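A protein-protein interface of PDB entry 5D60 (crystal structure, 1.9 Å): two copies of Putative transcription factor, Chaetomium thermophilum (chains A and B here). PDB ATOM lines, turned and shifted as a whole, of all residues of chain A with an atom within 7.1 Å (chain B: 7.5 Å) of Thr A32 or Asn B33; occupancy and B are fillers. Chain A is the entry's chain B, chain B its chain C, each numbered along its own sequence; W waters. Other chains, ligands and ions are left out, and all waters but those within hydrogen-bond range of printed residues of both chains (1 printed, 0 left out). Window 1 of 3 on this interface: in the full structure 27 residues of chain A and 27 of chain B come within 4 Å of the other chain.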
ATOM      1  N   CYS A  26      20.487  11.442  32.611  1.00  0.00           N
ATOM      2  CA  CYS A  26      19.304  11.157  33.407  1.00  0.00           C
ATOM      3  C   CYS A  26      17.988  11.476  32.646  1.00  0.00           C
ATOM      4  O   CYS A  26      16.972  10.781  32.832  1.00  0.00           O
ATOM      5  CB  CYS A  26      19.412  11.886  34.714  1.00  0.00           C
ATOM      6  SG  CYS A  26      20.624  11.099  35.820  1.00  0.00           S
ATOM      7  N   TYR A  27      17.999  12.487  31.798  1.00  0.00           N
ATOM      8  CA  TYR A  27      16.818  12.789  30.965  1.00  0.00           C
ATOM      9  C   TYR A  27      16.561  11.669  30.041  1.00  0.00           C
ATOM     10  O   TYR A  27      15.421  11.299  29.843  1.00  0.00           O
ATOM     11  CB  TYR A  27      16.948  14.058  30.129  1.00  0.00           C
ATOM     12  CG  TYR A  27      17.013  15.404  30.910  1.00  0.00           C
ATOM     13  CD1 TYR A  27      16.141  15.688  31.971  1.00  0.00           C
ATOM     14  CD2 TYR A  27      17.938  16.405  30.541  1.00  0.00           C
ATOM     15  CE1 TYR A  27      16.200  16.896  32.642  1.00  0.00           C
ATOM     16  CE2 TYR A  27      18.009  17.617  31.217  1.00  0.00           C
ATOM     17  CZ  TYR A  27      17.140  17.863  32.255  1.00  0.00           C
ATOM     18  OH  TYR A  27      17.233  19.075  32.894  1.00  0.00           O
ATOM     19  N   GLU A  28      17.613  11.095  29.455  1.00  0.00           N
ATOM     20  CA  GLU A  28      17.471   9.995  28.557  1.00  0.00           C
ATOM     21  C   GLU A  28      16.934   8.735  29.282  1.00  0.00           C
ATOM     22  O   GLU A  28      16.095   7.990  28.717  1.00  0.00           O
ATOM     23  CB  GLU A  28      18.798   9.669  27.838  1.00  0.00           C
ATOM     24  CG  GLU A  28      19.554  10.748  27.082  1.00  0.00           C
ATOM     25  CD  GLU A  28      18.924  11.227  25.773  1.00  0.00           C
ATOM     26  OE1 GLU A  28      17.796  10.769  25.427  1.00  0.00           O
ATOM     27  OE2 GLU A  28      19.607  12.073  25.111  1.00  0.00           O
ATOM     28  N   LEU A  29      17.329   8.509  30.524  1.00  0.00           N
ATOM     29  CA  LEU A  29      16.760   7.431  31.313  1.00  0.00           C
ATOM     30  C   LEU A  29      15.305   7.653  31.616  1.00  0.00           C
ATOM     31  O   LEU A  29      14.575   6.726  31.591  1.00  0.00           O
ATOM     32  CB  LEU A  29      17.503   7.298  32.644  1.00  0.00           C
ATOM     33  CG  LEU A  29      18.897   6.632  32.591  1.00  0.00           C
ATOM     34  CD1 LEU A  29      19.467   6.675  34.003  1.00  0.00           C
ATOM     35  CD2 LEU A  29      18.827   5.216  32.076  1.00  0.00           C
ATOM     36  N   GLU A  30      14.916   8.893  31.888  1.00  0.00           N
ATOM     37  CA  GLU A  30      13.525   9.207  32.129  1.00  0.00           C
ATOM     38  C   GLU A  30      12.684   8.889  30.954  1.00  0.00           C
ATOM     39  O   GLU A  30      11.592   8.318  31.115  1.00  0.00           O
ATOM     40  CB  GLU A  30      13.370  10.721  32.450  1.00  0.00           C
ATOM     41  CG  GLU A  30      13.663  11.078  33.862  1.00  0.00           C
ATOM     42  CD  GLU A  30      13.589  12.557  34.030  1.00  0.00           C
ATOM     43  OE1 GLU A  30      12.446  13.099  34.111  1.00  0.00           O
ATOM     44  OE2 GLU A  30      14.687  13.126  34.067  1.00  0.00           O
ATOM     45  N   LYS A  31      13.152   9.274  29.773  1.00  0.00           N
ATOM     46  CA  LYS A  31      12.458   9.009  28.539  1.00  0.00           C
ATOM     47  C   LYS A  31      12.222   7.559  28.326  1.00  0.00           C
ATOM     48  O   LYS A  31      11.082   7.110  28.068  1.00  0.00           O
ATOM     49  CB  LYS A  31      13.264   9.544  27.362  1.00  0.00           C
ATOM     50  CG  LYS A  31      12.597   9.399  25.993  1.00  0.00           C
ATOM     51  CD  LYS A  31      13.526   9.766  24.873  1.00  0.00           C
ATOM     52  CE  LYS A  31      14.622   8.709  24.785  1.00  0.00           C
ATOM     53  NZ  LYS A  31      15.585   8.994  23.709  1.00  0.00           N
ATOM     54  N   THR A  32      13.264   6.747  28.424  1.00  0.00           N
ATOM     55  CA  THR A  32      13.069   5.337  28.219  1.00  0.00           C
ATOM     56  C   THR A  32      12.261   4.662  29.353  1.00  0.00           C
ATOM     57  O   THR A  32      11.598   3.726  29.085  1.00  0.00           O
ATOM     58  CB  THR A  32      14.352   4.558  27.858  1.00  0.00           C
ATOM     59  OG1 THR A  32      15.331   4.838  28.840  1.00  0.00           O
ATOM     60  CG2 THR A  32      14.887   5.123  26.607  1.00  0.00           C
ATOM     61  N   ASN A  33      12.418   5.057  30.611  1.00  0.00           N
ATOM     62  CA  ASN A  33      11.534   4.578  31.644  1.00  0.00           C
ATOM     63  C   ASN A  33      10.094   4.860  31.266  1.00  0.00           C
ATOM     64  O   ASN A  33       9.243   4.038  31.487  1.00  0.00           O
ATOM     65  CB  ASN A  33      11.810   5.216  33.002  1.00  0.00           C
ATOM     66  CG  ASN A  33      12.912   4.503  33.800  1.00  0.00           C
ATOM     67  OD1 ASN A  33      13.589   3.591  33.313  1.00  0.00           O
ATOM     68  ND2 ASN A  33      13.112   4.954  35.022  1.00  0.00           N
ATOM     69  N   ARG A  34       9.820   6.047  30.778  1.00  0.00           N
ATOM     70  CA  ARG A  34       8.413   6.377  30.445  1.00  0.00           C
ATOM     71  C   ARG A  34       7.910   5.413  29.389  1.00  0.00           C
ATOM     72  O   ARG A  34       6.751   5.003  29.392  1.00  0.00           O
ATOM     73  CB  ARG A  34       8.322   7.762  29.841  1.00  0.00           C
ATOM     74  CG  ARG A  34       7.267   8.633  30.423  1.00  0.00           C
ATOM     75  CD  ARG A  34       5.910   8.128  29.959  1.00  0.00           C
ATOM     76  NE  ARG A  34       4.847   9.126  29.807  1.00  0.00           N
ATOM     77  CZ  ARG A  34       4.818  10.107  28.901  1.00  0.00           C
ATOM     78  NH1 ARG A  34       5.835  10.333  28.070  1.00  0.00           N
ATOM     79  NH2 ARG A  34       3.761  10.903  28.849  1.00  0.00           N
ATOM     80  N   LEU A  35       8.774   5.094  28.426  1.00  0.00           N
ATOM     81  CA  LEU A  35       8.415   4.174  27.394  1.00  0.00           C
ATOM     82  C   LEU A  35       8.133   2.826  28.003  1.00  0.00           C
ATOM     83  O   LEU A  35       7.147   2.206  27.710  1.00  0.00           O
ATOM     84  CB  LEU A  35       9.521   3.991  26.342  1.00  0.00           C
ATOM     85  CG  LEU A  35       9.816   5.040  25.331  1.00  0.00           C
ATOM     86  CD1 LEU A  35      10.680   4.371  24.255  1.00  0.00           C
ATOM     87  CD2 LEU A  35       8.630   5.798  24.703  1.00  0.00           C
ATOM     88  N   LEU A  36       9.014   2.377  28.906  1.00  0.00           N
ATOM     89  CA  LEU A  36       8.832   1.118  29.527  1.00  0.00           C
ATOM     90  C   LEU A  36       7.541   1.051  30.343  1.00  0.00           C
ATOM     91  O   LEU A  36       6.793   0.084  30.217  1.00  0.00           O
ATOM     92  CB  LEU A  36      10.015   0.770  30.433  1.00  0.00           C
ATOM     93  CG  LEU A  36      11.287   0.242  29.763  1.00  0.00           C
ATOM     94  CD1 LEU A  36      12.503   0.283  30.707  1.00  0.00           C
ATOM     95  CD2 LEU A  36      11.096  -1.173  29.226  1.00  0.00           C
ATOM     96  N   VAL A  37       7.226   2.105  31.074  1.00  0.00           N
ATOM     97  CA  VAL A  37       6.008   2.048  31.871  1.00  0.00           C
ATOM     98  C   VAL A  37       4.823   1.774  30.918  1.00  0.00           C
ATOM     99  O   VAL A  37       4.076   0.853  31.102  1.00  0.00           O
ATOM    100  CB  VAL A  37       5.802   3.326  32.655  1.00  0.00           C
ATOM    101  CG1 VAL A  37       4.379   3.398  33.213  1.00  0.00           C
ATOM    102  CG2 VAL A  37       6.842   3.435  33.726  1.00  0.00           C
ATOM    103  N   SER A  38       4.751   2.553  29.851  1.00  0.00           N
ATOM    104  CA  SER A  38       3.692   2.443  28.875  1.00  0.00           C
ATOM    105  C   SER A  38       3.640   1.094  28.236  1.00  0.00           C
ATOM    106  O   SER A  38       2.605   0.458  28.161  1.00  0.00           O
ATOM    107  CB  SER A  38       3.907   3.552  27.796  1.00  0.00           C
ATOM    108  OG  SER A  38       2.988   3.487  26.737  1.00  0.00           O
ATOM    109  N   TYR B  27      25.546   5.629  31.625  1.00  0.00           N
ATOM    110  CA  TYR B  27      25.563   5.057  30.308  1.00  0.00           C
ATOM    111  C   TYR B  27      25.166   3.614  30.236  1.00  0.00           C
ATOM    112  O   TYR B  27      24.418   3.236  29.362  1.00  0.00           O
ATOM    113  CB  TYR B  27      26.947   5.336  29.698  1.00  0.00           C
ATOM    114  CG  TYR B  27      27.141   4.617  28.412  1.00  0.00           C
ATOM    115  CD1 TYR B  27      26.384   4.964  27.302  1.00  0.00           C
ATOM    116  CD2 TYR B  27      28.132   3.648  28.277  1.00  0.00           C
ATOM    117  CE1 TYR B  27      26.572   4.338  26.085  1.00  0.00           C
ATOM    118  CE2 TYR B  27      28.316   2.984  27.078  1.00  0.00           C
ATOM    119  CZ  TYR B  27      27.576   3.370  25.969  1.00  0.00           C
ATOM    120  OH  TYR B  27      27.723   2.633  24.838  1.00  0.00           O
ATOM    121  N   GLU B  28      25.628   2.784  31.150  1.00  0.00           N
ATOM    122  CA  GLU B  28      25.284   1.429  31.186  1.00  0.00           C
ATOM    123  C   GLU B  28      23.788   1.258  31.553  1.00  0.00           C
ATOM    124  O   GLU B  28      23.138   0.409  31.042  1.00  0.00           O
ATOM    125  CB  GLU B  28      26.184   0.694  32.202  1.00  0.00           C
ATOM    126  CG  GLU B  28      27.676   0.670  31.811  1.00  0.00           C
ATOM    127  CD  GLU B  28      27.978  -0.127  30.536  1.00  0.00           C
ATOM    128  OE1 GLU B  28      27.173  -1.004  30.132  1.00  0.00           O
ATOM    129  OE2 GLU B  28      29.046   0.126  29.927  1.00  0.00           O
ATOM    130  N   LEU B  29      23.265   2.160  32.348  1.00  0.00           N
ATOM    131  CA  LEU B  29      21.841   2.076  32.601  1.00  0.00           C
ATOM    132  C   LEU B  29      20.991   2.475  31.373  1.00  0.00           C
ATOM    133  O   LEU B  29      19.989   1.897  31.152  1.00  0.00           O
ATOM    134  CB  LEU B  29      21.534   3.032  33.791  1.00  0.00           C
ATOM    135  CG  LEU B  29      21.909   2.620  35.219  1.00  0.00           C
ATOM    136  CD1 LEU B  29      21.441   3.738  36.152  1.00  0.00           C
ATOM    137  CD2 LEU B  29      21.248   1.321  35.631  1.00  0.00           C
ATOM    138  N   GLU B  30      21.434   3.463  30.631  1.00  0.00           N
ATOM    139  CA  GLU B  30      20.812   3.878  29.357  1.00  0.00           C
ATOM    140  C   GLU B  30      20.768   2.777  28.350  1.00  0.00           C
ATOM    141  O   GLU B  30      19.727   2.498  27.795  1.00  0.00           O
ATOM    142  CB  GLU B  30      21.570   5.037  28.765  1.00  0.00           C
ATOM    143  CG  GLU B  30      21.333   6.420  29.388  1.00  0.00           C
ATOM    144  CD  GLU B  30      22.304   7.491  28.878  1.00  0.00           C
ATOM    145  OE1 GLU B  30      23.553   7.356  29.080  1.00  0.00           O
ATOM    146  OE2 GLU B  30      21.827   8.509  28.275  1.00  0.00           O
ATOM    147  N   LYS B  31      21.878   2.028  28.226  1.00  0.00           N
ATOM    148  CA  LYS B  31      21.965   0.868  27.400  1.00  0.00           C
ATOM    149  C   LYS B  31      20.998  -0.218  27.766  1.00  0.00           C
ATOM    150  O   LYS B  31      20.252  -0.763  26.955  1.00  0.00           O
ATOM    151  CB  LYS B  31      23.419   0.313  27.491  1.00  0.00           C
ATOM    152  CG  LYS B  31      24.400   1.102  26.678  1.00  0.00           C
ATOM    153  CD  LYS B  31      25.841   0.732  26.972  1.00  0.00           C
ATOM    154  CE  LYS B  31      26.163  -0.647  26.472  1.00  0.00           C
ATOM    155  NZ  LYS B  31      27.577  -1.032  26.774  1.00  0.00           N
ATOM    156  N   THR B  32      21.000  -0.550  29.028  1.00  0.00           N
ATOM    157  CA  THR B  32      20.106  -1.531  29.555  1.00  0.00           C
ATOM    158  C   THR B  32      18.647  -1.132  29.402  1.00  0.00           C
ATOM    159  O   THR B  32      17.873  -1.976  29.027  1.00  0.00           O
ATOM    160  CB  THR B  32      20.448  -1.835  31.046  1.00  0.00           C
ATOM    161  OG1 THR B  32      21.763  -2.400  31.102  1.00  0.00           O
ATOM    162  CG2 THR B  32      19.558  -2.829  31.603  1.00  0.00           C
ATOM    163  N   ASN B  33      18.274   0.094  29.687  1.00  0.00           N
ATOM    164  CA  ASN B  33      16.904   0.483  29.328  1.00  0.00           C
ATOM    165  C   ASN B  33      16.505   0.273  27.831  1.00  0.00           C
ATOM    166  O   ASN B  33      15.428  -0.185  27.522  1.00  0.00           O
ATOM    167  CB  ASN B  33      16.652   1.932  29.701  1.00  0.00           C
ATOM    168  CG  ASN B  33      16.020   2.040  31.101  1.00  0.00           C
ATOM    169  OD1 ASN B  33      16.280   1.189  31.973  1.00  0.00           O
ATOM    170  ND2 ASN B  33      15.222   3.078  31.327  1.00  0.00           N
ATOM    171  N   ARG B  34      17.420   0.565  26.909  1.00  0.00           N
ATOM    172  CA  ARG B  34      17.137   0.398  25.519  1.00  0.00           C
ATOM    173  C   ARG B  34      16.906  -1.065  25.174  1.00  0.00           C
ATOM    174  O   ARG B  34      16.074  -1.430  24.359  1.00  0.00           O
ATOM    175  CB  ARG B  34      18.231   1.063  24.628  1.00  0.00           C
ATOM    176  CG  ARG B  34      18.052   2.514  24.440  1.00  0.00           C
ATOM    177  CD  ARG B  34      19.031   3.106  23.410  1.00  0.00           C
ATOM    178  NE  ARG B  34      20.453   2.971  23.752  1.00  0.00           N
ATOM    179  CZ  ARG B  34      21.160   3.823  24.528  1.00  0.00           C
ATOM    180  NH1 ARG B  34      20.587   4.886  25.121  1.00  0.00           N
ATOM    181  NH2 ARG B  34      22.450   3.628  24.705  1.00  0.00           N
ATOM    182  N   LEU B  35      17.668  -1.951  25.810  1.00  0.00           N
ATOM    183  CA  LEU B  35      17.502  -3.310  25.652  1.00  0.00           C
ATOM    184  C   LEU B  35      16.154  -3.790  26.241  1.00  0.00           C
ATOM    185  O   LEU B  35      15.439  -4.535  25.617  1.00  0.00           O
ATOM    186  CB  LEU B  35      18.675  -4.037  26.370  1.00  0.00           C
ATOM    187  CG  LEU B  35      18.576  -5.560  26.409  1.00  0.00           C
ATOM    188  CD1 LEU B  35      18.615  -6.147  25.002  1.00  0.00           C
ATOM    189  CD2 LEU B  35      19.687  -6.164  27.263  1.00  0.00           C
ATOM    190  N   LEU B  36      15.786  -3.246  27.384  1.00  0.00           N
ATOM    191  CA  LEU B  36      14.542  -3.628  27.974  1.00  0.00           C
ATOM    192  C   LEU B  36      13.406  -3.277  27.005  1.00  0.00           C
ATOM    193  O   LEU B  36      12.420  -4.027  26.913  1.00  0.00           O
ATOM    194  CB  LEU B  36      14.439  -3.033  29.364  1.00  0.00           C
ATOM    195  CG  LEU B  36      15.221  -3.731  30.549  1.00  0.00           C
ATOM    196  CD1 LEU B  36      15.307  -2.840  31.765  1.00  0.00           C
ATOM    197  CD2 LEU B  36      14.600  -5.044  30.923  1.00  0.00           C
ATOM    198  N   VAL B  37      13.487  -2.112  26.411  1.00  0.00           N
ATOM    199  CA  VAL B  37      12.407  -1.634  25.519  1.00  0.00           C
ATOM    200  C   VAL B  37      12.214  -2.645  24.419  1.00  0.00           C
ATOM    201  O   VAL B  37      11.107  -3.105  24.095  1.00  0.00           O
ATOM    202  CB  VAL B  37      12.693  -0.192  25.028  1.00  0.00           C
ATOM    203  CG1 VAL B  37      11.813   0.175  23.814  1.00  0.00           C
ATOM    204  CG2 VAL B  37      12.551   0.846  26.135  1.00  0.00           C
ATOM    205  N   SER B  38      13.299  -3.046  23.789  1.00  0.00           N
ATOM    206  CA  SER B  38      13.236  -4.021  22.797  1.00  0.00           C
ATOM    207  C   SER B  38      12.606  -5.291  23.261  1.00  0.00           C
ATOM    208  O   SER B  38      11.889  -5.905  22.545  1.00  0.00           O
ATOM    209  CB  SER B  38      14.664  -4.239  22.124  1.00  0.00           C
ATOM    210  OG  SER B  38      15.545  -5.067  22.902  1.00  0.00           O
ATOM    211  N   GLU B  39      12.979  -5.781  24.445  1.00  0.00           N
ATOM    212  CA  GLU B  39      12.492  -7.057  24.935  1.00  0.00           C
ATOM    213  C   GLU B  39      10.983  -6.950  25.143  1.00  0.00           C
ATOM    214  O   GLU B  39      10.217  -7.834  24.743  1.00  0.00           O
ATOM    215  CB  GLU B  39      13.111  -7.340  26.274  1.00  0.00           C
ATOM    216  CG  GLU B  39      14.609  -7.730  26.282  1.00  0.00           C
ATOM    217  CD  GLU B  39      14.919  -9.045  25.570  1.00  0.00           C
ATOM    218  OE1 GLU B  39      14.037  -9.956  25.514  1.00  0.00           O
ATOM    219  OE2 GLU B  39      16.076  -9.138  25.068  1.00  0.00           O
HETATM  220  O   HOH W   1      17.894   4.577  27.713  1.00  0.00           O
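The side-chain amide nitrogen (ND2) of Asn B33 sits at hydrogen-bond distance from the side-chain amide oxygen (OD1) of Asn A33 (2.6 Å).
ND2 of Asn B33 sits at hydrogen-bond distance from OG1 of Thr A32, 3.0 Å away.
Leu B29 touches its own counterpart, Leu A29.
Leu A29 touches Glu B30, but with the chains exchanged Glu A30 does not touch Leu B29 (8.7 Å).
Leu A29 touches Asn B33, but with the chains exchanged Asn A33 does not touch Leu B29 (7.0 Å).
Leu A36 touches Val B37, but with the chains exchanged Val A37 does not touch Leu B36 (9.0 Å).
Glu A28 touches Glu B30 (CB to OE2, 3.3 Å).
C of Leu B29 touches CD2 of Leu A29, at 3.6 Å.
Leu A29 touches Glu B30 (CD2 to N, 3.5 Å).
ND2 of Asn B33 touches O of Leu A29, at 3.7 Å.
Asn B33 touches Leu A36.
CD2 of Leu A36 touches CB of Leu B36 (3.8 Å).
N of Val B37 touches CD2 of Leu A36, at 3.8 Å.
Water W1 lies within hydrogen-bond range of the backbone carbonyl oxygen of Glu B30 (2.8 Å) and the side-chain hydroxyl of Thr A32 (2.8 Å).
Of the 13 printed residues of chain A, 5 touch a printed residue of chain B.
Hydrophobic or aromatic side chains of chain A that line the printed part of chain B: Leu A29 and Leu A36.
Along chain A the printed residues that touch a printed residue of chain B span positions 28 to 36.
Along chain B the printed residues that touch a printed residue of chain A span positions 29 to 37.
Among the printed residues, no Asp or Glu carboxylate lies within 4 Å of a Lys or Arg side-chain nitrogen of the other chain.
OE1 of Glu A28 lies within salt-bridge range of NZ of Lys A31, at 3.3 Å.
The backbone carbonyl oxygen (O) of Leu A29 lies within hydrogen-bond range of the side-chain hydroxyl (OG1) of Thr A32 (3.4 Å).
O of Glu A28 lies within hydrogen-bond range of OG1 of Thr A32, 3.2 Å away.
Of the printed residues of chain B, Glu A28 touches Glu B30 (3.3 Å).
Printed residues of chain A within 4 Å of Leu B36: Leu A36.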
